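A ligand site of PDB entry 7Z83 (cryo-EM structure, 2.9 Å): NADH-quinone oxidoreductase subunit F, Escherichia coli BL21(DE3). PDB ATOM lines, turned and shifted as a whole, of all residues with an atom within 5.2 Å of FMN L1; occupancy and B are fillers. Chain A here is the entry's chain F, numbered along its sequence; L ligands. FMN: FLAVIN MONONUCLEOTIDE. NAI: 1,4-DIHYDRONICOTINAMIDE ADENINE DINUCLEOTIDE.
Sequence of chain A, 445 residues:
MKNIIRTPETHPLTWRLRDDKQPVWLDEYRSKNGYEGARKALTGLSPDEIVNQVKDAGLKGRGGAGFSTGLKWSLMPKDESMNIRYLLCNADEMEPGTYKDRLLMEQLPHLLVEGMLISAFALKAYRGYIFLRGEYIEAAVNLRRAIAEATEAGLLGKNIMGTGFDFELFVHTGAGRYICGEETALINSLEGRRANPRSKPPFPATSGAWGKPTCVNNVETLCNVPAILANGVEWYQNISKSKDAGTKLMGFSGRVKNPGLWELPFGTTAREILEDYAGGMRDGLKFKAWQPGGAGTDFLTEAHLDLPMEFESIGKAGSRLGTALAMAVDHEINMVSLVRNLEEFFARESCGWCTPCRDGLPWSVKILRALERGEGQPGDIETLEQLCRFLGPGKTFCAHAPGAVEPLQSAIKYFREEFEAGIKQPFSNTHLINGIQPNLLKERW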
ATOM      1  N   GLY A  61      29.809  18.934  -2.933  1.00  0.00           N
ATOM      2  CA  GLY A  61      28.759  17.928  -2.976  1.00  0.00           C
ATOM      3  C   GLY A  61      28.422  17.404  -1.588  1.00  0.00           C
ATOM      4  O   GLY A  61      29.296  16.936  -0.865  1.00  0.00           O
ATOM      5  N   ARG A  62      27.140  17.490  -1.226  1.00  0.00           N
ATOM      6  CA  ARG A  62      26.666  17.008   0.062  1.00  0.00           C
ATOM      7  C   ARG A  62      26.287  15.537   0.030  1.00  0.00           C
ATOM      8  O   ARG A  62      25.798  15.024   1.041  1.00  0.00           O
ATOM      9  CB  ARG A  62      25.466  17.842   0.519  1.00  0.00           C
ATOM     10  CG  ARG A  62      25.747  19.328   0.624  1.00  0.00           C
ATOM     11  CD  ARG A  62      26.891  19.585   1.578  1.00  0.00           C
ATOM     12  NE  ARG A  62      26.881  20.958   2.088  1.00  0.00           N
ATOM     13  CZ  ARG A  62      27.705  21.913   1.678  1.00  0.00           C
ATOM     14  NH1 ARG A  62      28.610  21.685   0.750  1.00  0.00           N
ATOM     15  NH2 ARG A  62      27.612  23.126   2.222  1.00  0.00           N
ATOM     16  N   GLY A  63      26.493  14.858  -1.097  1.00  0.00           N
ATOM     17  CA  GLY A  63      26.241  13.433  -1.160  1.00  0.00           C
ATOM     18  C   GLY A  63      27.169  12.627  -0.273  1.00  0.00           C
ATOM     19  O   GLY A  63      26.762  11.609   0.301  1.00  0.00           O
ATOM     20  N   GLY A  64      28.416  13.072  -0.121  1.00  0.00           N
ATOM     21  CA  GLY A  64      29.349  12.387   0.736  1.00  0.00           C
ATOM     22  C   GLY A  64      30.772  12.393   0.204  1.00  0.00           C
ATOM     23  O   GLY A  64      31.704  11.994   0.913  1.00  0.00           O
ATOM     24  N   ALA A  65      30.948  12.843  -1.029  1.00  0.00           N
ATOM     25  CA  ALA A  65      32.270  12.872  -1.655  1.00  0.00           C
ATOM     26  C   ALA A  65      32.946  14.231  -1.577  1.00  0.00           C
ATOM     27  O   ALA A  65      34.183  14.283  -1.582  1.00  0.00           O
ATOM     28  CB  ALA A  65      32.165  12.452  -3.123  1.00  0.00           C
ATOM     29  N   PHE A  67      32.789  16.697  -3.833  1.00  0.00           N
ATOM     30  CA  PHE A  67      33.136  17.266  -5.127  1.00  0.00           C
ATOM     31  C   PHE A  67      32.467  18.619  -5.303  1.00  0.00           C
ATOM     32  O   PHE A  67      31.347  18.856  -4.848  1.00  0.00           O
ATOM     33  CB  PHE A  67      32.729  16.325  -6.260  1.00  0.00           C
ATOM     34  CG  PHE A  67      33.429  16.603  -7.559  1.00  0.00           C
ATOM     35  CD1 PHE A  67      34.738  16.194  -7.760  1.00  0.00           C
ATOM     36  CD2 PHE A  67      32.770  17.249  -8.588  1.00  0.00           C
ATOM     37  CE1 PHE A  67      35.380  16.451  -8.956  1.00  0.00           C
ATOM     38  CE2 PHE A  67      33.403  17.509  -9.787  1.00  0.00           C
ATOM     39  CZ  PHE A  67      34.709  17.110  -9.971  1.00  0.00           C
ATOM     40  N   THR A  69      30.357  21.416  -6.692  1.00  0.00           N
ATOM     41  CA  THR A  69      29.142  21.422  -7.505  1.00  0.00           C
ATOM     42  C   THR A  69      29.278  22.345  -8.705  1.00  0.00           C
ATOM     43  O   THR A  69      28.805  22.020  -9.796  1.00  0.00           O
ATOM     44  CB  THR A  69      27.939  21.812  -6.653  1.00  0.00           C
ATOM     45  OG1 THR A  69      27.977  21.079  -5.426  1.00  0.00           O
ATOM     46  CG2 THR A  69      26.652  21.511  -7.383  1.00  0.00           C
ATOM     47  N   LYS A  72      31.393  20.595 -11.232  1.00  0.00           N
ATOM     48  CA  LYS A  72      30.605  19.578 -11.908  1.00  0.00           C
ATOM     49  C   LYS A  72      29.620  20.190 -12.899  1.00  0.00           C
ATOM     50  O   LYS A  72      29.326  19.591 -13.939  1.00  0.00           O
ATOM     51  CB  LYS A  72      29.852  18.736 -10.881  1.00  0.00           C
ATOM     52  CG  LYS A  72      29.376  17.391 -11.410  1.00  0.00           C
ATOM     53  CD  LYS A  72      28.128  16.926 -10.679  1.00  0.00           C
ATOM     54  CE  LYS A  72      28.422  16.670  -9.214  1.00  0.00           C
ATOM     55  NZ  LYS A  72      27.356  15.853  -8.586  1.00  0.00           N
ATOM     56  N   ASN A  90      19.267  13.125  -6.346  1.00  0.00           N
ATOM     57  CA  ASN A  90      19.542  11.829  -5.744  1.00  0.00           C
ATOM     58  C   ASN A  90      18.915  11.793  -4.353  1.00  0.00           C
ATOM     59  O   ASN A  90      19.571  12.003  -3.331  1.00  0.00           O
ATOM     60  CB  ASN A  90      21.048  11.581  -5.687  1.00  0.00           C
ATOM     61  CG  ASN A  90      21.396  10.122  -5.549  1.00  0.00           C
ATOM     62  OD1 ASN A  90      20.641   9.342  -4.975  1.00  0.00           O
ATOM     63  ND2 ASN A  90      22.553   9.737  -6.065  1.00  0.00           N
ATOM     64  N   ASP A  92      17.764   9.077  -3.068  1.00  0.00           N
ATOM     65  CA  ASP A  92      17.773   7.681  -2.646  1.00  0.00           C
ATOM     66  C   ASP A  92      18.061   7.574  -1.160  1.00  0.00           C
ATOM     67  O   ASP A  92      17.210   7.123  -0.382  1.00  0.00           O
ATOM     68  CB  ASP A  92      18.797   6.884  -3.454  1.00  0.00           C
ATOM     69  CG  ASP A  92      18.408   5.435  -3.627  1.00  0.00           C
ATOM     70  OD1 ASP A  92      17.202   5.135  -3.606  1.00  0.00           O
ATOM     71  OD2 ASP A  92      19.315   4.591  -3.761  1.00  0.00           O
ATOM     72  N   GLU A  93      19.254   8.015  -0.739  1.00  0.00           N
ATOM     73  CA  GLU A  93      19.658   8.106   0.676  1.00  0.00           C
ATOM     74  C   GLU A  93      19.505   6.759   1.396  1.00  0.00           C
ATOM     75  O   GLU A  93      18.875   6.659   2.449  1.00  0.00           O
ATOM     76  CB  GLU A  93      18.881   9.201   1.398  1.00  0.00           C
ATOM     77  CG  GLU A  93      19.653   9.856   2.527  1.00  0.00           C
ATOM     78  CD  GLU A  93      18.751  10.364   3.626  1.00  0.00           C
ATOM     79  OE1 GLU A  93      17.654   9.806   3.814  1.00  0.00           O
ATOM     80  OE2 GLU A  93      19.145  11.331   4.323  1.00  0.00           O
ATOM     81  N   MET A  94      20.083   5.727   0.803  1.00  0.00           N
ATOM     82  CA  MET A  94      19.955   4.373   1.334  1.00  0.00           C
ATOM     83  C   MET A  94      21.108   3.983   2.240  1.00  0.00           C
ATOM     84  O   MET A  94      21.165   2.823   2.671  1.00  0.00           O
ATOM     85  CB  MET A  94      19.857   3.380   0.172  1.00  0.00           C
ATOM     86  CG  MET A  94      18.503   3.364  -0.509  1.00  0.00           C
ATOM     87  SD  MET A  94      17.566   1.879  -0.134  1.00  0.00           S
ATOM     88  CE  MET A  94      16.310   1.976  -1.391  1.00  0.00           C
ATOM     89  N   GLU A  95      22.004   4.903   2.540  1.00  0.00           N
ATOM     90  CA  GLU A  95      23.117   4.611   3.442  1.00  0.00           C
ATOM     91  C   GLU A  95      22.608   4.441   4.863  1.00  0.00           C
ATOM     92  O   GLU A  95      21.806   5.262   5.336  1.00  0.00           O
ATOM     93  CB  GLU A  95      24.158   5.719   3.391  1.00  0.00           C
ATOM     94  CG  GLU A  95      25.304   5.565   4.375  1.00  0.00           C
ATOM     95  CD  GLU A  95      26.515   4.920   3.759  1.00  0.00           C
ATOM     96  OE1 GLU A  95      26.378   3.814   3.197  1.00  0.00           O
ATOM     97  OE2 GLU A  95      27.613   5.511   3.832  1.00  0.00           O
ATOM     98  N   ASP A 101      18.198  13.737   4.331  1.00  0.00           N
ATOM     99  CA  ASP A 101      17.382  14.108   3.186  1.00  0.00           C
ATOM    100  C   ASP A 101      15.898  13.895   3.457  1.00  0.00           C
ATOM    101  O   ASP A 101      15.072  14.621   2.917  1.00  0.00           O
ATOM    102  CB  ASP A 101      17.825  13.316   1.953  1.00  0.00           C
ATOM    103  CG  ASP A 101      19.266  13.584   1.571  1.00  0.00           C
ATOM    104  OD1 ASP A 101      19.790  14.645   1.966  1.00  0.00           O
ATOM    105  OD2 ASP A 101      19.873  12.748   0.866  1.00  0.00           O
ATOM    106  N   TYR A 178      20.017  -0.442  -2.736  1.00  0.00           N
ATOM    107  CA  TYR A 178      20.965   0.545  -2.229  1.00  0.00           C
ATOM    108  C   TYR A 178      21.903   1.063  -3.315  1.00  0.00           C
ATOM    109  O   TYR A 178      22.302   2.228  -3.274  1.00  0.00           O
ATOM    110  CB  TYR A 178      21.772  -0.068  -1.080  1.00  0.00           C
ATOM    111  CG  TYR A 178      23.047   0.668  -0.697  1.00  0.00           C
ATOM    112  CD1 TYR A 178      23.001   1.776   0.113  1.00  0.00           C
ATOM    113  CD2 TYR A 178      24.289   0.219  -1.124  1.00  0.00           C
ATOM    114  CE1 TYR A 178      24.150   2.445   0.480  1.00  0.00           C
ATOM    115  CE2 TYR A 178      25.442   0.878  -0.774  1.00  0.00           C
ATOM    116  CZ  TYR A 178      25.366   1.990   0.028  1.00  0.00           C
ATOM    117  OH  TYR A 178      26.511   2.646   0.390  1.00  0.00           O
ATOM    118  N   ILE A 179      22.232   0.223  -4.291  1.00  0.00           N
ATOM    119  CA  ILE A 179      23.173   0.618  -5.344  1.00  0.00           C
ATOM    120  C   ILE A 179      22.568   1.688  -6.257  1.00  0.00           C
ATOM    121  O   ILE A 179      23.318   2.368  -6.963  1.00  0.00           O
ATOM    122  CB  ILE A 179      23.616  -0.634  -6.125  1.00  0.00           C
ATOM    123  CG1 ILE A 179      24.904  -0.370  -6.923  1.00  0.00           C
ATOM    124  CG2 ILE A 179      22.514  -1.132  -7.030  1.00  0.00           C
ATOM    125  CD1 ILE A 179      25.976   0.367  -6.145  1.00  0.00           C
ATOM    126  N   GLY A 181      21.625   4.527  -5.498  1.00  0.00           N
ATOM    127  CA  GLY A 181      22.108   5.847  -5.138  1.00  0.00           C
ATOM    128  C   GLY A 181      23.362   6.271  -5.869  1.00  0.00           C
ATOM    129  O   GLY A 181      23.631   7.465  -5.978  1.00  0.00           O
ATOM    130  N   GLU A 182      24.152   5.307  -6.346  1.00  0.00           N
ATOM    131  CA  GLU A 182      25.273   5.613  -7.228  1.00  0.00           C
ATOM    132  C   GLU A 182      24.759   6.255  -8.502  1.00  0.00           C
ATOM    133  O   GLU A 182      23.804   5.752  -9.114  1.00  0.00           O
ATOM    134  CB  GLU A 182      26.037   4.328  -7.558  1.00  0.00           C
ATOM    135  CG  GLU A 182      27.539   4.491  -7.682  1.00  0.00           C
ATOM    136  CD  GLU A 182      27.972   4.907  -9.070  1.00  0.00           C
ATOM    137  OE1 GLU A 182      27.259   4.570 -10.035  1.00  0.00           O
ATOM    138  OE2 GLU A 182      29.023   5.572  -9.188  1.00  0.00           O
ATOM    139  N   GLU A 183      25.390   7.365  -8.913  1.00  0.00           N
ATOM    140  CA  GLU A 183      24.761   8.250  -9.892  1.00  0.00           C
ATOM    141  C   GLU A 183      24.652   7.608 -11.273  1.00  0.00           C
ATOM    142  O   GLU A 183      23.674   7.832 -11.990  1.00  0.00           O
ATOM    143  CB  GLU A 183      25.511   9.586  -9.970  1.00  0.00           C
ATOM    144  CG  GLU A 183      26.823   9.550 -10.737  1.00  0.00           C
ATOM    145  CD  GLU A 183      27.557  10.851 -10.683  1.00  0.00           C
ATOM    146  OE1 GLU A 183      28.628  10.918 -11.317  1.00  0.00           O
ATOM    147  OE2 GLU A 183      27.079  11.797 -10.032  1.00  0.00           O
ATOM    148  N   VAL A 216      23.752  14.872 -11.849  1.00  0.00           N
ATOM    149  CA  VAL A 216      23.171  14.234 -10.675  1.00  0.00           C
ATOM    150  C   VAL A 216      23.689  14.941  -9.434  1.00  0.00           C
ATOM    151  O   VAL A 216      24.909  15.088  -9.263  1.00  0.00           O
ATOM    152  CB  VAL A 216      23.508  12.731 -10.631  1.00  0.00           C
ATOM    153  CG1 VAL A 216      22.625  12.035  -9.620  1.00  0.00           C
ATOM    154  CG2 VAL A 216      23.355  12.109 -11.999  1.00  0.00           C
ATOM    155  N   ASN A 217      22.774  15.384  -8.570  1.00  0.00           N
ATOM    156  CA  ASN A 217      23.154  16.109  -7.370  1.00  0.00           C
ATOM    157  C   ASN A 217      22.286  15.681  -6.201  1.00  0.00           C
ATOM    158  O   ASN A 217      21.140  15.272  -6.386  1.00  0.00           O
ATOM    159  CB  ASN A 217      23.059  17.622  -7.574  1.00  0.00           C
ATOM    160  CG  ASN A 217      24.340  18.228  -8.096  1.00  0.00           C
ATOM    161  OD1 ASN A 217      24.379  18.738  -9.207  1.00  0.00           O
ATOM    162  ND2 ASN A 217      25.386  18.172  -7.294  1.00  0.00           N
ATOM    163  N   ASN A 218      22.839  15.779  -5.001  1.00  0.00           N
ATOM    164  CA  ASN A 218      22.139  15.379  -3.786  1.00  0.00           C
ATOM    165  C   ASN A 218      21.035  16.385  -3.461  1.00  0.00           C
ATOM    166  O   ASN A 218      20.969  17.495  -3.995  1.00  0.00           O
ATOM    167  CB  ASN A 218      23.123  15.260  -2.626  1.00  0.00           C
ATOM    168  CG  ASN A 218      22.560  14.458  -1.461  1.00  0.00           C
ATOM    169  OD1 ASN A 218      21.549  13.773  -1.603  1.00  0.00           O
ATOM    170  ND2 ASN A 218      23.206  14.550  -0.318  1.00  0.00           N
ATOM    171  N   THR A 221      22.585  19.521  -1.523  1.00  0.00           N
ATOM    172  CA  THR A 221      23.263  20.477  -2.386  1.00  0.00           C
ATOM    173  C   THR A 221      22.272  21.405  -3.074  1.00  0.00           C
ATOM    174  O   THR A 221      22.435  22.634  -3.075  1.00  0.00           O
ATOM    175  CB  THR A 221      24.108  19.731  -3.425  1.00  0.00           C
ATOM    176  OG1 THR A 221      24.962  18.791  -2.761  1.00  0.00           O
ATOM    177  CG2 THR A 221      24.950  20.699  -4.199  1.00  0.00           C
ATOM    178  N   CYS A 398      32.925  -0.076  -8.930  1.00  0.00           N
ATOM    179  CA  CYS A 398      32.388   1.142  -8.338  1.00  0.00           C
ATOM    180  C   CYS A 398      32.869   1.245  -6.901  1.00  0.00           C
ATOM    181  O   CYS A 398      33.591   0.365  -6.404  1.00  0.00           O
ATOM    182  CB  CYS A 398      30.865   1.180  -8.446  1.00  0.00           C
ATOM    183  SG  CYS A 398      29.969   0.456  -7.074  1.00  0.00           S
ATOM    184  N   ALA A 399      32.468   2.318  -6.221  1.00  0.00           N
ATOM    185  CA  ALA A 399      32.972   2.633  -4.896  1.00  0.00           C
ATOM    186  C   ALA A 399      32.138   2.043  -3.769  1.00  0.00           C
ATOM    187  O   ALA A 399      32.262   2.490  -2.626  1.00  0.00           O
ATOM    188  CB  ALA A 399      33.074   4.158  -4.724  1.00  0.00           C
ATOM    189  N   HIS A 400      31.303   1.052  -4.063  1.00  0.00           N
ATOM    190  CA  HIS A 400      30.483   0.430  -3.021  1.00  0.00           C
ATOM    191  C   HIS A 400      31.331  -0.454  -2.109  1.00  0.00           C
ATOM    192  O   HIS A 400      31.191  -0.409  -0.885  1.00  0.00           O
ATOM    193  CB  HIS A 400      29.352  -0.368  -3.674  1.00  0.00           C
ATOM    194  CG  HIS A 400      28.746  -1.411  -2.793  1.00  0.00           C
ATOM    195  ND1 HIS A 400      29.202  -2.708  -2.767  1.00  0.00           N
ATOM    196  CD2 HIS A 400      27.713  -1.351  -1.919  1.00  0.00           C
ATOM    197  CE1 HIS A 400      28.473  -3.400  -1.910  1.00  0.00           C
ATOM    198  NE2 HIS A 400      27.566  -2.607  -1.388  1.00  0.00           N
HETATM  199  N1  FMN L   1      24.440   9.970  -3.207  1.00  0.00           N
HETATM  200  C2  FMN L   1      23.198  10.350  -2.766  1.00  0.00           C
HETATM  201  O2  FMN L   1      22.890  11.538  -2.780  1.00  0.00           O
HETATM  202  N3  FMN L   1      22.315   9.407  -2.293  1.00  0.00           N
HETATM  203  C4  FMN L   1      22.675   8.085  -2.287  1.00  0.00           C
HETATM  204  O4  FMN L   1      21.892   7.230  -1.875  1.00  0.00           O
HETATM  205  C4A FMN L   1      23.921   7.695  -2.745  1.00  0.00           C
HETATM  206  N5  FMN L   1      24.288   6.375  -2.726  1.00  0.00           N
HETATM  207  C5A FMN L   1      25.523   5.993  -3.179  1.00  0.00           C
HETATM  208  C6  FMN L   1      25.867   4.652  -3.154  1.00  0.00           C
HETATM  209  C7  FMN L   1      27.103   4.246  -3.606  1.00  0.00           C
HETATM  210  C7M FMN L   1      27.454   2.791  -3.574  1.00  0.00           C
HETATM  211  C8  FMN L   1      28.010   5.185  -4.082  1.00  0.00           C
HETATM  212  C8M FMN L   1      29.372   4.764  -4.566  1.00  0.00           C
HETATM  213  C9  FMN L   1      27.665   6.531  -4.099  1.00  0.00           C
HETATM  214  C9A FMN L   1      26.420   6.941  -3.651  1.00  0.00           C
HETATM  215  N10 FMN L   1      26.061   8.282  -3.668  1.00  0.00           N
HETATM  216  C10 FMN L   1      24.815   8.648  -3.208  1.00  0.00           C
HETATM  217  C1' FMN L   1      27.004   9.340  -4.167  1.00  0.00           C
HETATM  218  C2' FMN L   1      26.737   9.607  -5.655  1.00  0.00           C
HETATM  219  O2' FMN L   1      27.591   8.800  -6.437  1.00  0.00           O
HETATM  220  C3' FMN L   1      26.958  11.065  -6.036  1.00  0.00           C
HETATM  221  O3' FMN L   1      28.189  11.492  -5.505  1.00  0.00           O
HETATM  222  C4' FMN L   1      25.831  11.933  -5.477  1.00  0.00           C
HETATM  223  O4' FMN L   1      24.614  11.238  -5.589  1.00  0.00           O
HETATM  224  C5' FMN L   1      25.702  13.275  -6.176  1.00  0.00           C
HETATM  225  O5' FMN L   1      26.893  14.002  -6.028  1.00  0.00           O
HETATM  226  P   FMN L   1      26.911  15.359  -5.155  1.00  0.00           P
HETATM  227  O1P FMN L   1      27.482  15.023  -3.804  1.00  0.00           O
HETATM  228  O2P FMN L   1      27.763  16.395  -5.836  1.00  0.00           O
HETATM  229  O3P FMN L   1      25.513  15.881  -4.990  1.00  0.00           O
HETATM  230  PA  NAI L   2      33.404  10.276  -6.649  1.00  0.00           P
HETATM  231  O1A NAI L   2      33.981  10.998  -5.497  1.00  0.00           O
HETATM  232  O2A NAI L   2      34.414   9.888  -7.721  1.00  0.00           O
HETATM  233  O5B NAI L   2      32.276  11.148  -7.372  1.00  0.00           O
HETATM  234  C5B NAI L   2      31.471  12.132  -6.689  1.00  0.00           C
HETATM  235  C4B NAI L   2      30.957  13.142  -7.675  1.00  0.00           C
HETATM  236  O4B NAI L   2      32.064  13.815  -8.320  1.00  0.00           O
HETATM  237  C3B NAI L   2      30.080  12.579  -8.797  1.00  0.00           C
HETATM  238  O3B NAI L   2      28.947  13.408  -9.032  1.00  0.00           O
HETATM  239  C2B NAI L   2      31.033  12.556 -10.001  1.00  0.00           C
HETATM  240  O2B NAI L   2      30.326  12.701 -11.230  1.00  0.00           O
HETATM  241  C1B NAI L   2      31.898  13.772  -9.720  1.00  0.00           C
HETATM  242  N9A NAI L   2      33.214  13.707 -10.341  1.00  0.00           N
HETATM  243  C8A NAI L   2      34.351  13.143  -9.820  1.00  0.00           C
HETATM  244  N7A NAI L   2      35.397  13.256 -10.589  1.00  0.00           N
HETATM  245  C5A NAI L   2      34.931  13.937 -11.698  1.00  0.00           C
HETATM  246  C6A NAI L   2      35.550  14.374 -12.882  1.00  0.00           C
HETATM  247  N6A NAI L   2      36.843  14.180 -13.159  1.00  0.00           N
HETATM  248  N1A NAI L   2      34.794  15.027 -13.797  1.00  0.00           N
HETATM  249  C2A NAI L   2      33.493  15.225 -13.524  1.00  0.00           C
HETATM  250  N3A NAI L   2      32.801  14.863 -12.445  1.00  0.00           N
HETATM  251  C4A NAI L   2      33.577  14.220 -11.566  1.00  0.00           C
HETATM  252  O3  NAI L   2      32.694   8.927  -6.182  1.00  0.00           O
HETATM  253  PN  NAI L   2      31.207   8.372  -6.141  1.00  0.00           P
HETATM  254  O1N NAI L   2      31.287   6.860  -6.314  1.00  0.00           O
HETATM  255  O2N NAI L   2      30.313   9.042  -7.097  1.00  0.00           O
HETATM  256  O5D NAI L   2      30.726   8.620  -4.629  1.00  0.00           O
HETATM  257  C5D NAI L   2      31.481   8.186  -3.486  1.00  0.00           C
HETATM  258  C4D NAI L   2      30.921   8.860  -2.261  1.00  0.00           C
HETATM  259  O4D NAI L   2      29.555   8.462  -2.083  1.00  0.00           O
HETATM  260  C3D NAI L   2      31.629   8.524  -0.951  1.00  0.00           C
HETATM  261  O3D NAI L   2      32.521   9.557  -0.562  1.00  0.00           O
HETATM  262  C2D NAI L   2      30.485   8.339   0.069  1.00  0.00           C
HETATM  263  O2D NAI L   2      30.623   9.215   1.189  1.00  0.00           O
HETATM  264  C1D NAI L   2      29.225   8.702  -0.730  1.00  0.00           C
HETATM  265  N1N NAI L   2      28.067   7.884  -0.389  1.00  0.00           N
HETATM  266  C2N NAI L   2      26.858   8.484  -0.026  1.00  0.00           C
HETATM  267  C3N NAI L   2      25.755   7.773   0.292  1.00  0.00           C
HETATM  268  C7N NAI L   2      24.539   8.529   0.659  1.00  0.00           C
HETATM  269  O7N NAI L   2      24.577   9.759   0.805  1.00  0.00           O
HETATM  270  N7N NAI L   2      23.420   7.835   0.848  1.00  0.00           N
HETATM  271  C4N NAI L   2      25.787   6.276   0.263  1.00  0.00           C
HETATM  272  C5N NAI L   2      27.120   5.748  -0.100  1.00  0.00           C
HETATM  273  C6N NAI L   2      28.149   6.525  -0.401  1.00  0.00           C
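O of Asn 90 sits close to OD1 of Asn 218, 3.2 Å away.
O of Gly 181 is in hydrogen-bond range of ND2 of Asn 90 (2.5 Å).
The backbone carbonyl oxygen (O) of Asn 217 sits at hydrogen-bond distance from the backbone NH (N) of Asn 90 (2.8 Å).
The backbone NH (N) of Asp 92 lies close to the side-chain amide oxygen (OD1) of Asn 90, at 3.5 Å.
The backbone NH (N) of Asp 101 sits at hydrogen-bond distance from the side-chain carboxylate (OE2) of Glu 93 (2.6 Å).
N of Gly 181 is in hydrogen-bond range of OD2 of Asp 92 (2.9 Å).
The backbone NH of Gly 61 is in hydrogen-bond range of the backbone carbonyl oxygen of Phe 67, 2.5 Å away.
The backbone NH (N) of Arg 62 sits at hydrogen-bond distance from the side-chain hydroxyl (OG1) of Thr 221 (3.0 Å).
The side-chain amide nitrogen of Asn 90 sits at hydrogen-bond distance from an oxygen (O4') of FMN L1.
O3P of FMN L1 sits at hydrogen-bond distance from N of Asn 218, at 2.7 Å.
O2 of FMN L1 lies close to OD1 of Asn 218, at 2.9 Å.
O2P of FMN L1 lies within salt-bridge range of NZ of Lys 72 (2.8 Å).
The backbone NH of Gly 63 is in hydrogen-bond range of an oxygen (O1P) of FMN L1 (2.9 Å).
The backbone NH (N) of Glu 93 lies within hydrogen-bond range of an oxygen (O4) of FMN L1.
An oxygen (O3P) of FMN L1 is in hydrogen-bond range of the side-chain amide nitrogen (ND2) of Asn 217 (3.3 Å).
The side-chain amino group (NZ) of Lys 72 is in hydrogen-bond range of an oxygen (O3B) of NAI L2 (3.0 Å).
The side-chain carboxylate (OE1) of Glu 183 is in hydrogen-bond range of an oxygen (O2B) of NAI L2, 2.5 Å away.
O of Gly 64 lies within hydrogen-bond range of O3D of NAI L2 (3.0 Å).
An oxygen (O2') of FMN L1 sits at hydrogen-bond distance from an oxygen (O2N) of NAI L2, at 2.8 Å.
The backbone carbonyl oxygen (O) of Gly 181 lies close to a nitrogen (N10) of FMN L1 (3.5 Å).
Merely in contact with FMN L1: Gly 61, Arg 62, Asp 92, Met 94, Tyr 178, Ile 179, Glu 182, Glu 183, Val 216, Thr 221, Ala 399 and His 400.
The nearest printed residue that does not touch FMN L1 is Gly 64 (4.3 Å).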
